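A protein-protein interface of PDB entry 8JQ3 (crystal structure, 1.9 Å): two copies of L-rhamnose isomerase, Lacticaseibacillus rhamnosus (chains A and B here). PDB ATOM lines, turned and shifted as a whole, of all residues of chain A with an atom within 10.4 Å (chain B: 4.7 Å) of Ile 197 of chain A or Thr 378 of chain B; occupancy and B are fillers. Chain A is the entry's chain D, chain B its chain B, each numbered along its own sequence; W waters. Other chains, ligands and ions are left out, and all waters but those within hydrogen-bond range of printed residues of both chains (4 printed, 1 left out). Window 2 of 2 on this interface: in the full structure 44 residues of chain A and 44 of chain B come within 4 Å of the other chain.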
ATOM      1  N   MET A 147      10.637   1.430 -23.585  1.00  0.00           N
ATOM      2  CA  MET A 147      10.598   1.866 -25.003  1.00  0.00           C
ATOM      3  C   MET A 147       9.145   2.003 -25.464  1.00  0.00           C
ATOM      4  O   MET A 147       8.278   1.253 -24.967  1.00  0.00           O
ATOM      5  CB  MET A 147      11.358   0.884 -25.895  1.00  0.00           C
ATOM      6  CG  MET A 147      12.846   1.013 -25.756  1.00  0.00           C
ATOM      7  SD  MET A 147      13.723  -0.164 -26.790  1.00  0.00           S
ATOM      8  CE  MET A 147      15.416   0.289 -26.407  1.00  0.00           C
ATOM      9  N   GLY A 191      15.220   3.895 -24.241  1.00  0.00           N
ATOM     10  CA  GLY A 191      16.653   3.671 -23.976  1.00  0.00           C
ATOM     11  C   GLY A 191      16.907   2.380 -23.220  1.00  0.00           C
ATOM     12  O   GLY A 191      15.973   1.567 -23.101  1.00  0.00           O
ATOM     13  N   PHE A 192      18.133   2.201 -22.717  1.00  0.00           N
ATOM     14  CA  PHE A 192      18.554   0.994 -21.962  1.00  0.00           C
ATOM     15  C   PHE A 192      19.141   1.380 -20.602  1.00  0.00           C
ATOM     16  O   PHE A 192      19.874   2.369 -20.509  1.00  0.00           O
ATOM     17  CB  PHE A 192      19.636   0.197 -22.688  1.00  0.00           C
ATOM     18  CG  PHE A 192      19.204  -0.442 -23.983  1.00  0.00           C
ATOM     19  CD1 PHE A 192      18.482  -1.626 -23.995  1.00  0.00           C
ATOM     20  CD2 PHE A 192      19.573   0.122 -25.187  1.00  0.00           C
ATOM     21  CE1 PHE A 192      18.097  -2.207 -25.193  1.00  0.00           C
ATOM     22  CE2 PHE A 192      19.180  -0.456 -26.381  1.00  0.00           C
ATOM     23  CZ  PHE A 192      18.455  -1.622 -26.380  1.00  0.00           C
ATOM     24  N   LYS A 193      18.870   0.554 -19.601  1.00  0.00           N
ATOM     25  CA  LYS A 193      19.501   0.695 -18.263  1.00  0.00           C
ATOM     26  C   LYS A 193      21.006   0.429 -18.386  1.00  0.00           C
ATOM     27  O   LYS A 193      21.800   1.213 -17.825  1.00  0.00           O
ATOM     28  CB  LYS A 193      18.843  -0.254 -17.266  1.00  0.00           C
ATOM     29  CG  LYS A 193      19.495  -0.217 -15.890  1.00  0.00           C
ATOM     30  CD  LYS A 193      18.865  -1.125 -14.868  1.00  0.00           C
ATOM     31  CE  LYS A 193      19.562  -1.016 -13.527  1.00  0.00           C
ATOM     32  NZ  LYS A 193      18.626  -1.232 -12.400  1.00  0.00           N
ATOM     33  N   ASP A 194      21.388  -0.638 -19.091  1.00  0.00           N
ATOM     34  CA  ASP A 194      22.802  -1.075 -19.223  1.00  0.00           C
ATOM     35  C   ASP A 194      23.297  -0.921 -20.668  1.00  0.00           C
ATOM     36  O   ASP A 194      22.493  -0.542 -21.545  1.00  0.00           O
ATOM     37  CB  ASP A 194      22.976  -2.508 -18.725  1.00  0.00           C
ATOM     38  CG  ASP A 194      24.220  -2.682 -17.865  1.00  0.00           C
ATOM     39  OD1 ASP A 194      25.298  -2.236 -18.309  1.00  0.00           O
ATOM     40  OD2 ASP A 194      24.098  -3.253 -16.761  1.00  0.00           O
ATOM     41  N   ASN A 195      24.579  -1.220 -20.898  1.00  0.00           N
ATOM     42  CA  ASN A 195      25.296  -0.926 -22.169  1.00  0.00           C
ATOM     43  C   ASN A 195      24.667  -1.718 -23.313  1.00  0.00           C
ATOM     44  O   ASN A 195      24.551  -2.937 -23.232  1.00  0.00           O
ATOM     45  CB  ASN A 195      26.793  -1.200 -22.042  1.00  0.00           C
ATOM     46  CG  ASN A 195      27.466  -0.297 -21.030  1.00  0.00           C
ATOM     47  OD1 ASN A 195      27.296   0.921 -21.059  1.00  0.00           O
ATOM     48  ND2 ASN A 195      28.247  -0.884 -20.142  1.00  0.00           N
ATOM     49  N   PRO A 196      24.234  -1.049 -24.406  1.00  0.00           N
ATOM     50  CA  PRO A 196      23.660  -1.757 -25.543  1.00  0.00           C
ATOM     51  C   PRO A 196      24.721  -2.255 -26.531  1.00  0.00           C
ATOM     52  O   PRO A 196      25.831  -1.744 -26.544  1.00  0.00           O
ATOM     53  CB  PRO A 196      22.799  -0.668 -26.182  1.00  0.00           C
ATOM     54  CG  PRO A 196      23.634   0.570 -26.000  1.00  0.00           C
ATOM     55  CD  PRO A 196      24.236   0.409 -24.609  1.00  0.00           C
ATOM     56  N   ILE A 197      24.322  -3.227 -27.354  1.00  0.00           N
ATOM     57  CA  ILE A 197      25.138  -3.774 -28.469  1.00  0.00           C
ATOM     58  C   ILE A 197      24.850  -2.918 -29.700  1.00  0.00           C
ATOM     59  O   ILE A 197      25.790  -2.552 -30.421  1.00  0.00           O
ATOM     60  CB  ILE A 197      24.777  -5.250 -28.707  1.00  0.00           C
ATOM     61  CG1 ILE A 197      24.871  -6.051 -27.408  1.00  0.00           C
ATOM     62  CG2 ILE A 197      25.649  -5.839 -29.803  1.00  0.00           C
ATOM     63  CD1 ILE A 197      26.277  -6.196 -26.910  1.00  0.00           C
ATOM     64  N   ASP A 198      23.579  -2.601 -29.910  1.00  0.00           N
ATOM     65  CA  ASP A 198      23.129  -1.893 -31.129  1.00  0.00           C
ATOM     66  C   ASP A 198      22.593  -0.510 -30.765  1.00  0.00           C
ATOM     67  O   ASP A 198      21.484  -0.436 -30.267  1.00  0.00           O
ATOM     68  CB  ASP A 198      22.102  -2.742 -31.878  1.00  0.00           C
ATOM     69  CG  ASP A 198      21.761  -2.194 -33.246  1.00  0.00           C
ATOM     70  OD1 ASP A 198      21.938  -0.979 -33.450  1.00  0.00           O
ATOM     71  OD2 ASP A 198      21.320  -2.997 -34.081  1.00  0.00           O
ATOM     72  N   LYS A 199      23.357   0.530 -31.081  1.00  0.00           N
ATOM     73  CA  LYS A 199      22.967   1.945 -30.884  1.00  0.00           C
ATOM     74  C   LYS A 199      22.285   2.490 -32.141  1.00  0.00           C
ATOM     75  O   LYS A 199      21.570   3.491 -32.051  1.00  0.00           O
ATOM     76  CB  LYS A 199      24.222   2.760 -30.586  1.00  0.00           C
ATOM     77  CG  LYS A 199      24.979   2.301 -29.343  1.00  0.00           C
ATOM     78  CD  LYS A 199      26.110   3.209 -29.006  1.00  0.00           C
ATOM     79  CE  LYS A 199      26.744   2.883 -27.668  1.00  0.00           C
ATOM     80  NZ  LYS A 199      27.951   3.710 -27.457  1.00  0.00           N
ATOM     81  N   LYS A 200      22.544   1.868 -33.282  1.00  0.00           N
ATOM     82  CA  LYS A 200      22.072   2.402 -34.582  1.00  0.00           C
ATOM     83  C   LYS A 200      20.579   2.111 -34.774  1.00  0.00           C
ATOM     84  O   LYS A 200      19.845   3.055 -35.076  1.00  0.00           O
ATOM     85  CB  LYS A 200      22.912   1.805 -35.707  1.00  0.00           C
ATOM     86  CG  LYS A 200      22.284   1.939 -37.078  1.00  0.00           C
ATOM     87  CD  LYS A 200      23.230   1.560 -38.171  1.00  0.00           C
ATOM     88  CE  LYS A 200      23.342   0.067 -38.322  1.00  0.00           C
ATOM     89  NZ  LYS A 200      23.943  -0.270 -39.630  1.00  0.00           N
ATOM     90  N   THR A 201      20.152   0.856 -34.625  1.00  0.00           N
ATOM     91  CA  THR A 201      18.811   0.388 -35.063  1.00  0.00           C
ATOM     92  C   THR A 201      17.727   1.101 -34.255  1.00  0.00           C
ATOM     93  O   THR A 201      16.717   1.518 -34.815  1.00  0.00           O
ATOM     94  CB  THR A 201      18.728  -1.144 -35.082  1.00  0.00           C
ATOM     95  OG1 THR A 201      19.815  -1.648 -35.857  1.00  0.00           O
ATOM     96  CG2 THR A 201      17.432  -1.650 -35.675  1.00  0.00           C
ATOM     97  N   PRO A 202      17.874   1.293 -32.923  1.00  0.00           N
ATOM     98  CA  PRO A 202      16.887   2.067 -32.171  1.00  0.00           C
ATOM     99  C   PRO A 202      16.665   3.491 -32.705  1.00  0.00           C
ATOM    100  O   PRO A 202      15.552   3.958 -32.657  1.00  0.00           O
ATOM    101  CB  PRO A 202      17.478   2.115 -30.742  1.00  0.00           C
ATOM    102  CG  PRO A 202      18.325   0.862 -30.666  1.00  0.00           C
ATOM    103  CD  PRO A 202      18.916   0.714 -32.057  1.00  0.00           C
ATOM    104  N   ARG A 205      14.711   3.201 -35.956  1.00  0.00           N
ATOM    105  CA  ARG A 205      13.289   2.925 -35.636  1.00  0.00           C
ATOM    106  C   ARG A 205      12.634   4.234 -35.195  1.00  0.00           C
ATOM    107  O   ARG A 205      11.500   4.516 -35.658  1.00  0.00           O
ATOM    108  CB  ARG A 205      13.124   1.815 -34.598  1.00  0.00           C
ATOM    109  CG  ARG A 205      13.593   0.450 -35.073  1.00  0.00           C
ATOM    110  CD  ARG A 205      13.017  -0.655 -34.218  1.00  0.00           C
ATOM    111  NE  ARG A 205      13.397  -0.422 -32.824  1.00  0.00           N
ATOM    112  CZ  ARG A 205      14.395  -1.029 -32.201  1.00  0.00           C
ATOM    113  NH1 ARG A 205      15.114  -1.943 -32.826  1.00  0.00           N
ATOM    114  NH2 ARG A 205      14.673  -0.723 -30.944  1.00  0.00           N
ATOM    115  N   SER A 238      22.211   4.104 -19.217  1.00  0.00           N
ATOM    116  CA  SER A 238      23.373   3.815 -20.102  1.00  0.00           C
ATOM    117  C   SER A 238      23.153   4.286 -21.552  1.00  0.00           C
ATOM    118  O   SER A 238      24.145   4.539 -22.244  1.00  0.00           O
ATOM    119  CB  SER A 238      23.716   2.356 -20.075  1.00  0.00           C
ATOM    120  OG  SER A 238      24.142   1.950 -18.787  1.00  0.00           O
ATOM    121  N   TYR A 239      21.918   4.415 -22.013  1.00  0.00           N
ATOM    122  CA  TYR A 239      21.664   4.812 -23.429  1.00  0.00           C
ATOM    123  C   TYR A 239      20.275   5.419 -23.544  1.00  0.00           C
ATOM    124  O   TYR A 239      19.330   4.835 -23.001  1.00  0.00           O
ATOM    125  CB  TYR A 239      21.859   3.613 -24.359  1.00  0.00           C
ATOM    126  CG  TYR A 239      21.403   3.794 -25.790  1.00  0.00           C
ATOM    127  CD1 TYR A 239      22.283   4.162 -26.793  1.00  0.00           C
ATOM    128  CD2 TYR A 239      20.089   3.560 -26.146  1.00  0.00           C
ATOM    129  CE1 TYR A 239      21.866   4.303 -28.113  1.00  0.00           C
ATOM    130  CE2 TYR A 239      19.655   3.688 -27.458  1.00  0.00           C
ATOM    131  CZ  TYR A 239      20.545   4.066 -28.448  1.00  0.00           C
ATOM    132  OH  TYR A 239      20.130   4.190 -29.753  1.00  0.00           O
ATOM    133  N   ARG B 316      30.286  -2.746 -33.909  1.00  0.00           N
ATOM    134  CA  ARG B 316      28.959  -3.384 -33.699  1.00  0.00           C
ATOM    135  C   ARG B 316      27.911  -2.810 -34.664  1.00  0.00           C
ATOM    136  O   ARG B 316      27.002  -3.563 -35.016  1.00  0.00           O
ATOM    137  CB  ARG B 316      28.480  -3.205 -32.261  1.00  0.00           C
ATOM    138  CG  ARG B 316      29.265  -4.023 -31.247  1.00  0.00           C
ATOM    139  CD  ARG B 316      29.079  -3.477 -29.846  1.00  0.00           C
ATOM    140  NE  ARG B 316      29.698  -4.340 -28.853  1.00  0.00           N
ATOM    141  CZ  ARG B 316      29.529  -4.210 -27.550  1.00  0.00           C
ATOM    142  NH1 ARG B 316      28.764  -3.242 -27.081  1.00  0.00           N
ATOM    143  NH2 ARG B 316      30.121  -5.049 -26.719  1.00  0.00           N
ATOM    144  N   ASP B 317      27.988  -1.520 -35.005  1.00  0.00           N
ATOM    145  CA  ASP B 317      26.938  -0.823 -35.800  1.00  0.00           C
ATOM    146  C   ASP B 317      27.429  -0.632 -37.245  1.00  0.00           C
ATOM    147  O   ASP B 317      26.760   0.086 -38.011  1.00  0.00           O
ATOM    148  CB  ASP B 317      26.519   0.495 -35.140  1.00  0.00           C
ATOM    149  CG  ASP B 317      25.765   0.337 -33.825  1.00  0.00           C
ATOM    150  OD1 ASP B 317      24.945  -0.602 -33.711  1.00  0.00           O
ATOM    151  OD2 ASP B 317      25.996   1.168 -32.925  1.00  0.00           O
ATOM    152  N   ILE B 359      28.373 -10.842 -32.450  1.00  0.00           N
ATOM    153  CA  ILE B 359      27.582  -9.579 -32.501  1.00  0.00           C
ATOM    154  C   ILE B 359      26.147  -9.893 -32.944  1.00  0.00           C
ATOM    155  O   ILE B 359      25.219  -9.367 -32.305  1.00  0.00           O
ATOM    156  CB  ILE B 359      28.293  -8.532 -33.384  1.00  0.00           C
ATOM    157  CG1 ILE B 359      29.646  -8.145 -32.774  1.00  0.00           C
ATOM    158  CG2 ILE B 359      27.402  -7.317 -33.611  1.00  0.00           C
ATOM    159  CD1 ILE B 359      30.513  -7.265 -33.649  1.00  0.00           C
ATOM    160  N   LEU B 362      24.232 -11.594 -30.093  1.00  0.00           N
ATOM    161  CA  LEU B 362      24.082 -10.604 -28.996  1.00  0.00           C
ATOM    162  C   LEU B 362      22.975  -9.613 -29.370  1.00  0.00           C
ATOM    163  O   LEU B 362      22.157  -9.277 -28.500  1.00  0.00           O
ATOM    164  CB  LEU B 362      25.419  -9.897 -28.772  1.00  0.00           C
ATOM    165  CG  LEU B 362      26.411 -10.662 -27.902  1.00  0.00           C
ATOM    166  CD1 LEU B 362      27.759  -9.969 -27.904  1.00  0.00           C
ATOM    167  CD2 LEU B 362      25.884 -10.808 -26.480  1.00  0.00           C
ATOM    168  N   LYS B 363      22.947  -9.167 -30.624  1.00  0.00           N
ATOM    169  CA  LYS B 363      21.888  -8.251 -31.128  1.00  0.00           C
ATOM    170  C   LYS B 363      20.523  -8.921 -30.959  1.00  0.00           C
ATOM    171  O   LYS B 363      19.592  -8.244 -30.494  1.00  0.00           O
ATOM    172  CB  LYS B 363      22.134  -7.874 -32.593  1.00  0.00           C
ATOM    173  CG  LYS B 363      23.252  -6.869 -32.808  1.00  0.00           C
ATOM    174  CD  LYS B 363      23.493  -6.490 -34.251  1.00  0.00           C
ATOM    175  CE  LYS B 363      24.486  -5.355 -34.355  1.00  0.00           C
ATOM    176  NZ  LYS B 363      24.531  -4.772 -35.713  1.00  0.00           N
ATOM    177  N   GLU B 366      19.449  -9.021 -27.385  1.00  0.00           N
ATOM    178  CA  GLU B 366      19.089  -7.642 -26.979  1.00  0.00           C
ATOM    179  C   GLU B 366      17.691  -7.290 -27.508  1.00  0.00           C
ATOM    180  O   GLU B 366      16.911  -6.713 -26.739  1.00  0.00           O
ATOM    181  CB  GLU B 366      20.165  -6.689 -27.481  1.00  0.00           C
ATOM    182  CG  GLU B 366      19.876  -5.249 -27.157  1.00  0.00           C
ATOM    183  CD  GLU B 366      21.054  -4.350 -27.469  1.00  0.00           C
ATOM    184  OE1 GLU B 366      21.178  -3.952 -28.639  1.00  0.00           O
ATOM    185  OE2 GLU B 366      21.857  -4.084 -26.544  1.00  0.00           O
ATOM    186  N   ARG B 374      23.126 -10.697 -22.084  1.00  0.00           N
ATOM    187  CA  ARG B 374      23.978  -9.619 -22.650  1.00  0.00           C
ATOM    188  C   ARG B 374      25.050  -9.239 -21.622  1.00  0.00           C
ATOM    189  O   ARG B 374      26.241  -9.149 -21.988  1.00  0.00           O
ATOM    190  CB  ARG B 374      23.146  -8.398 -23.057  1.00  0.00           C
ATOM    191  CG  ARG B 374      23.964  -7.345 -23.789  1.00  0.00           C
ATOM    192  CD  ARG B 374      23.236  -6.035 -23.977  1.00  0.00           C
ATOM    193  NE  ARG B 374      22.754  -5.512 -22.709  1.00  0.00           N
ATOM    194  CZ  ARG B 374      21.772  -4.625 -22.592  1.00  0.00           C
ATOM    195  NH1 ARG B 374      21.165  -4.154 -23.669  1.00  0.00           N
ATOM    196  NH2 ARG B 374      21.390  -4.217 -21.400  1.00  0.00           N
ATOM    197  N   LEU B 375      24.650  -9.002 -20.378  1.00  0.00           N
ATOM    198  CA  LEU B 375      25.607  -8.620 -19.306  1.00  0.00           C
ATOM    199  C   LEU B 375      26.633  -9.746 -19.129  1.00  0.00           C
ATOM    200  O   LEU B 375      27.845  -9.456 -19.180  1.00  0.00           O
ATOM    201  CB  LEU B 375      24.853  -8.335 -18.008  1.00  0.00           C
ATOM    202  CG  LEU B 375      25.728  -7.839 -16.855  1.00  0.00           C
ATOM    203  CD1 LEU B 375      26.419  -6.534 -17.219  1.00  0.00           C
ATOM    204  CD2 LEU B 375      24.913  -7.676 -15.586  1.00  0.00           C
ATOM    205  N   ILE B 376      26.174 -10.987 -18.941  1.00  0.00           N
ATOM    206  CA  ILE B 376      27.072 -12.145 -18.654  1.00  0.00           C
ATOM    207  C   ILE B 376      28.087 -12.267 -19.795  1.00  0.00           C
ATOM    208  O   ILE B 376      29.291 -12.322 -19.500  1.00  0.00           O
ATOM    209  CB  ILE B 376      26.294 -13.458 -18.441  1.00  0.00           C
ATOM    210  CG1 ILE B 376      25.401 -13.415 -17.199  1.00  0.00           C
ATOM    211  CG2 ILE B 376      27.258 -14.630 -18.385  1.00  0.00           C
ATOM    212  CD1 ILE B 376      24.506 -14.617 -17.054  1.00  0.00           C
ATOM    213  N   GLU B 377      27.617 -12.287 -21.052  1.00  0.00           N
ATOM    214  CA  GLU B 377      28.475 -12.577 -22.231  1.00  0.00           C
ATOM    215  C   GLU B 377      29.468 -11.431 -22.464  1.00  0.00           C
ATOM    216  O   GLU B 377      30.658 -11.740 -22.641  1.00  0.00           O
ATOM    217  CB  GLU B 377      27.625 -12.869 -23.469  1.00  0.00           C
ATOM    218  CG  GLU B 377      27.050 -14.268 -23.450  1.00  0.00           C
ATOM    219  CD  GLU B 377      26.371 -14.706 -24.729  1.00  0.00           C
ATOM    220  OE1 GLU B 377      26.663 -14.117 -25.789  1.00  0.00           O
ATOM    221  OE2 GLU B 377      25.563 -15.643 -24.654  1.00  0.00           O
ATOM    222  N   THR B 378      29.023 -10.171 -22.472  1.00  0.00           N
ATOM    223  CA  THR B 378      29.918  -9.001 -22.704  1.00  0.00           C
ATOM    224  C   THR B 378      31.015  -8.980 -21.620  1.00  0.00           C
ATOM    225  O   THR B 378      32.165  -8.590 -21.923  1.00  0.00           O
ATOM    226  CB  THR B 378      29.138  -7.681 -22.794  1.00  0.00           C
ATOM    227  OG1 THR B 378      28.297  -7.517 -21.651  1.00  0.00           O
ATOM    228  CG2 THR B 378      28.303  -7.589 -24.054  1.00  0.00           C
ATOM    229  N   GLU B 379      30.696  -9.410 -20.403  1.00  0.00           N
ATOM    230  CA  GLU B 379      31.688  -9.423 -19.292  1.00  0.00           C
ATOM    231  C   GLU B 379      32.666 -10.589 -19.493  1.00  0.00           C
ATOM    232  O   GLU B 379      33.887 -10.367 -19.321  1.00  0.00           O
ATOM    233  CB  GLU B 379      30.970  -9.417 -17.944  1.00  0.00           C
ATOM    234  CG  GLU B 379      30.518  -8.022 -17.557  1.00  0.00           C
ATOM    235  CD  GLU B 379      31.587  -6.951 -17.713  1.00  0.00           C
ATOM    236  OE1 GLU B 379      32.653  -7.066 -17.051  1.00  0.00           O
ATOM    237  OE2 GLU B 379      31.353  -5.996 -18.488  1.00  0.00           O
ATOM    238  N   GLU B 380      32.173 -11.764 -19.895  1.00  0.00           N
ATOM    239  CA  GLU B 380      33.030 -12.952 -20.152  1.00  0.00           C
ATOM    240  C   GLU B 380      33.989 -12.648 -21.313  1.00  0.00           C
ATOM    241  O   GLU B 380      35.151 -13.092 -21.249  1.00  0.00           O
ATOM    242  CB  GLU B 380      32.184 -14.200 -20.422  1.00  0.00           C
ATOM    243  CG  GLU B 380      31.421 -14.700 -19.203  1.00  0.00           C
ATOM    244  CD  GLU B 380      32.236 -14.907 -17.935  1.00  0.00           C
ATOM    245  OE1 GLU B 380      33.418 -15.314 -18.037  1.00  0.00           O
ATOM    246  OE2 GLU B 380      31.678 -14.666 -16.846  1.00  0.00           O
ATOM    247  N   LEU B 381      33.542 -11.917 -22.337  1.00  0.00           N
ATOM    248  CA  LEU B 381      34.354 -11.695 -23.564  1.00  0.00           C
ATOM    249  C   LEU B 381      35.575 -10.843 -23.212  1.00  0.00           C
ATOM    250  O   LEU B 381      36.589 -10.940 -23.926  1.00  0.00           O
ATOM    251  CB  LEU B 381      33.498 -11.044 -24.656  1.00  0.00           C
ATOM    252  CG  LEU B 381      32.460 -11.961 -25.301  1.00  0.00           C
ATOM    253  CD1 LEU B 381      31.503 -11.158 -26.170  1.00  0.00           C
ATOM    254  CD2 LEU B 381      33.135 -13.055 -26.117  1.00  0.00           C
ATOM    255  N   LYS B 382      35.498 -10.060 -22.134  1.00  0.00           N
ATOM    256  CA  LYS B 382      36.615  -9.178 -21.704  1.00  0.00           C
ATOM    257  C   LYS B 382      37.806 -10.034 -21.267  1.00  0.00           C
ATOM    258  O   LYS B 382      38.931  -9.511 -21.317  1.00  0.00           O
ATOM    259  CB  LYS B 382      36.165  -8.211 -20.604  1.00  0.00           C
ATOM    260  CG  LYS B 382      35.220  -7.121 -21.093  1.00  0.00           C
ATOM    261  CD  LYS B 382      34.722  -6.200 -20.012  1.00  0.00           C
ATOM    262  CE  LYS B 382      33.878  -5.069 -20.557  1.00  0.00           C
ATOM    263  NZ  LYS B 382      33.328  -4.218 -19.475  1.00  0.00           N
HETATM  264  O   HOH W   1      27.227  -0.200 -30.736  1.00  0.00           O
HETATM  265  O   HOH W   2      28.107  -0.456 -28.179  1.00  0.00           O
HETATM  266  O   HOH W   3      26.041   0.898 -40.498  1.00  0.00           O
HETATM  267  O   HOH W   4      19.447  -2.196 -29.682  1.00  0.00           O
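No position is printed for both chains.
Of the 18 pairs that touch across the chains among the printed residues, none has its exchanged pair printed and touching as well.
The side-chain amino group (NZ) of Lys 363 of chain B sits at hydrogen-bond distance from the backbone carbonyl oxygen (O) of Arg 316 of chain B, 2.8 Å away.
The guanidinium group (NH1) of Arg 374 of chain B lies within salt-bridge range of the side-chain carboxylate (OE2) of Glu 366 of chain B, at 3.0 Å.
The backbone carbonyl oxygen of Arg 374 of chain B lies within hydrogen-bond range of the side-chain hydroxyl of Thr 378 of chain B (2.6 Å).
OG1 of Thr 378 of chain B sits at hydrogen-bond distance from O of Leu 375 of chain B (3.2 Å).
The backbone NH of Phe 192 of chain A sits at hydrogen-bond distance from the backbone carbonyl oxygen of Tyr 239 of chain A, 2.9 Å away.
The backbone NH of Lys 200 of chain A lies within hydrogen-bond range of the side-chain carboxylate of Asp 198 of chain A (2.9 Å).
NH1 of Arg 316 of chain B sits at hydrogen-bond distance from O of Pro 196 of chain A (3.3 Å).
The backbone NH (N) of Lys 199 of chain A lies within hydrogen-bond range of the side-chain carboxylate (OD1) of Asp 317 of chain B, at 3.3 Å.
The side-chain amino group of Lys 200 of chain A is in hydrogen-bond range of the backbone carbonyl oxygen of Asp 317 of chain B, at 3.3 Å.
OE2 of Glu 366 of chain B lies within hydrogen-bond range of N of Ile 197 of chain A, 2.7 Å away.
The side-chain carboxylate (OE1) of Glu 366 of chain B is in hydrogen-bond range of the backbone NH (N) of Asp 198 of chain A (3.0 Å).
The guanidinium group (NE) of Arg 374 of chain B sits at hydrogen-bond distance from the backbone carbonyl oxygen (O) of Asn 195 of chain A, at 3.2 Å.
OD1 of Asp 317 of chain B lies close to OD1 of Asp 198 of chain A (3.0 Å).
Water W3 bridges NZ of Lys 200 of chain A and O of Asp 317 of chain B.
Water W4 bridges OE1 of Glu 366 of chain B (2.7 Å) and O of Asp 198 of chain A (2.8 Å).
Water W1 lies within hydrogen-bond range of O of Ile 197 of chain A and OD2 of Asp 317 of chain B.
Water W2 lies within hydrogen-bond range of NH1 of Arg 316 of chain B (3.1 Å) and O of Pro 196 of chain A (3.1 Å).
Ile 197 of chain A touches six residues of chain B.
Of chain A, only Ile 197 (3.8 Å) comes within 4 Å of Thr 378 of chain B.
Arg 316 of chain B touches just these residues of chain A: Pro 196 and Ile 197.
No residue of chain A comes within 4 Å of Leu 362 of chain B.
Of the printed residues of chain A, Lys 363 of chain B touches Ile 197 and Asp 198.
Of the printed residues of chain A, Arg 374 of chain B touches Phe 192, Asp 194, Asn 195, Pro 196 and Ile 197.
Of the printed residues of chain B, Phe 192 of chain A touches Glu 366 (3.9 Å) and Arg 374 (3.7 Å).
Printed residues of chain B within 4 Å of Asn 195 of chain A: Arg 374.
Thr 201 of chain A touches none of the printed residues of chain B.
The nearest residue of chain A that does not touch Thr 378 of chain B is Asn 195 of chain A (6.0 Å).
Among the printed residues, merely in contact across the chains: Phe 192 of chain A with Glu 366 of chain B (3.9 Å), Phe 192 of chain A with Arg 374 of chain B (3.7 Å), Asp 194 of chain A with Arg 374 of chain B (3.5 Å), Pro 196 of chain A with Glu 366 of chain B (3.1 Å), Pro 196 of chain A with Arg 374 of chain B (3.9 Å), Ile 197 of chain A with Arg 316 of chain B (3.3 Å), Ile 197 of chain A with Asp 317 of chain B (3.9 Å), Ile 197 of chain A with Lys 363 of chain B (3.98 Å), Ile 197 of chain A with Arg 374 of chain B (3.8 Å), Ile 197 of chain A with Thr 378 of chain B (3.8 Å) and Asp 198 of chain A with Lys 363 of chain B (3.96 Å).
Printed residues of chain B that touch a printed residue of chain A: Arg 316, Asp 317, Lys 363, Glu 366, Arg 374 and Thr 378.
Of the 16 printed residues of chain A, 8 touch a printed residue of chain B.
Hydrophobic or aromatic side chains of chain A that line the printed part of chain B: Phe 192, Pro 196 and Ile 197.
Among the printed residues, 18 pairs touch across the chains.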
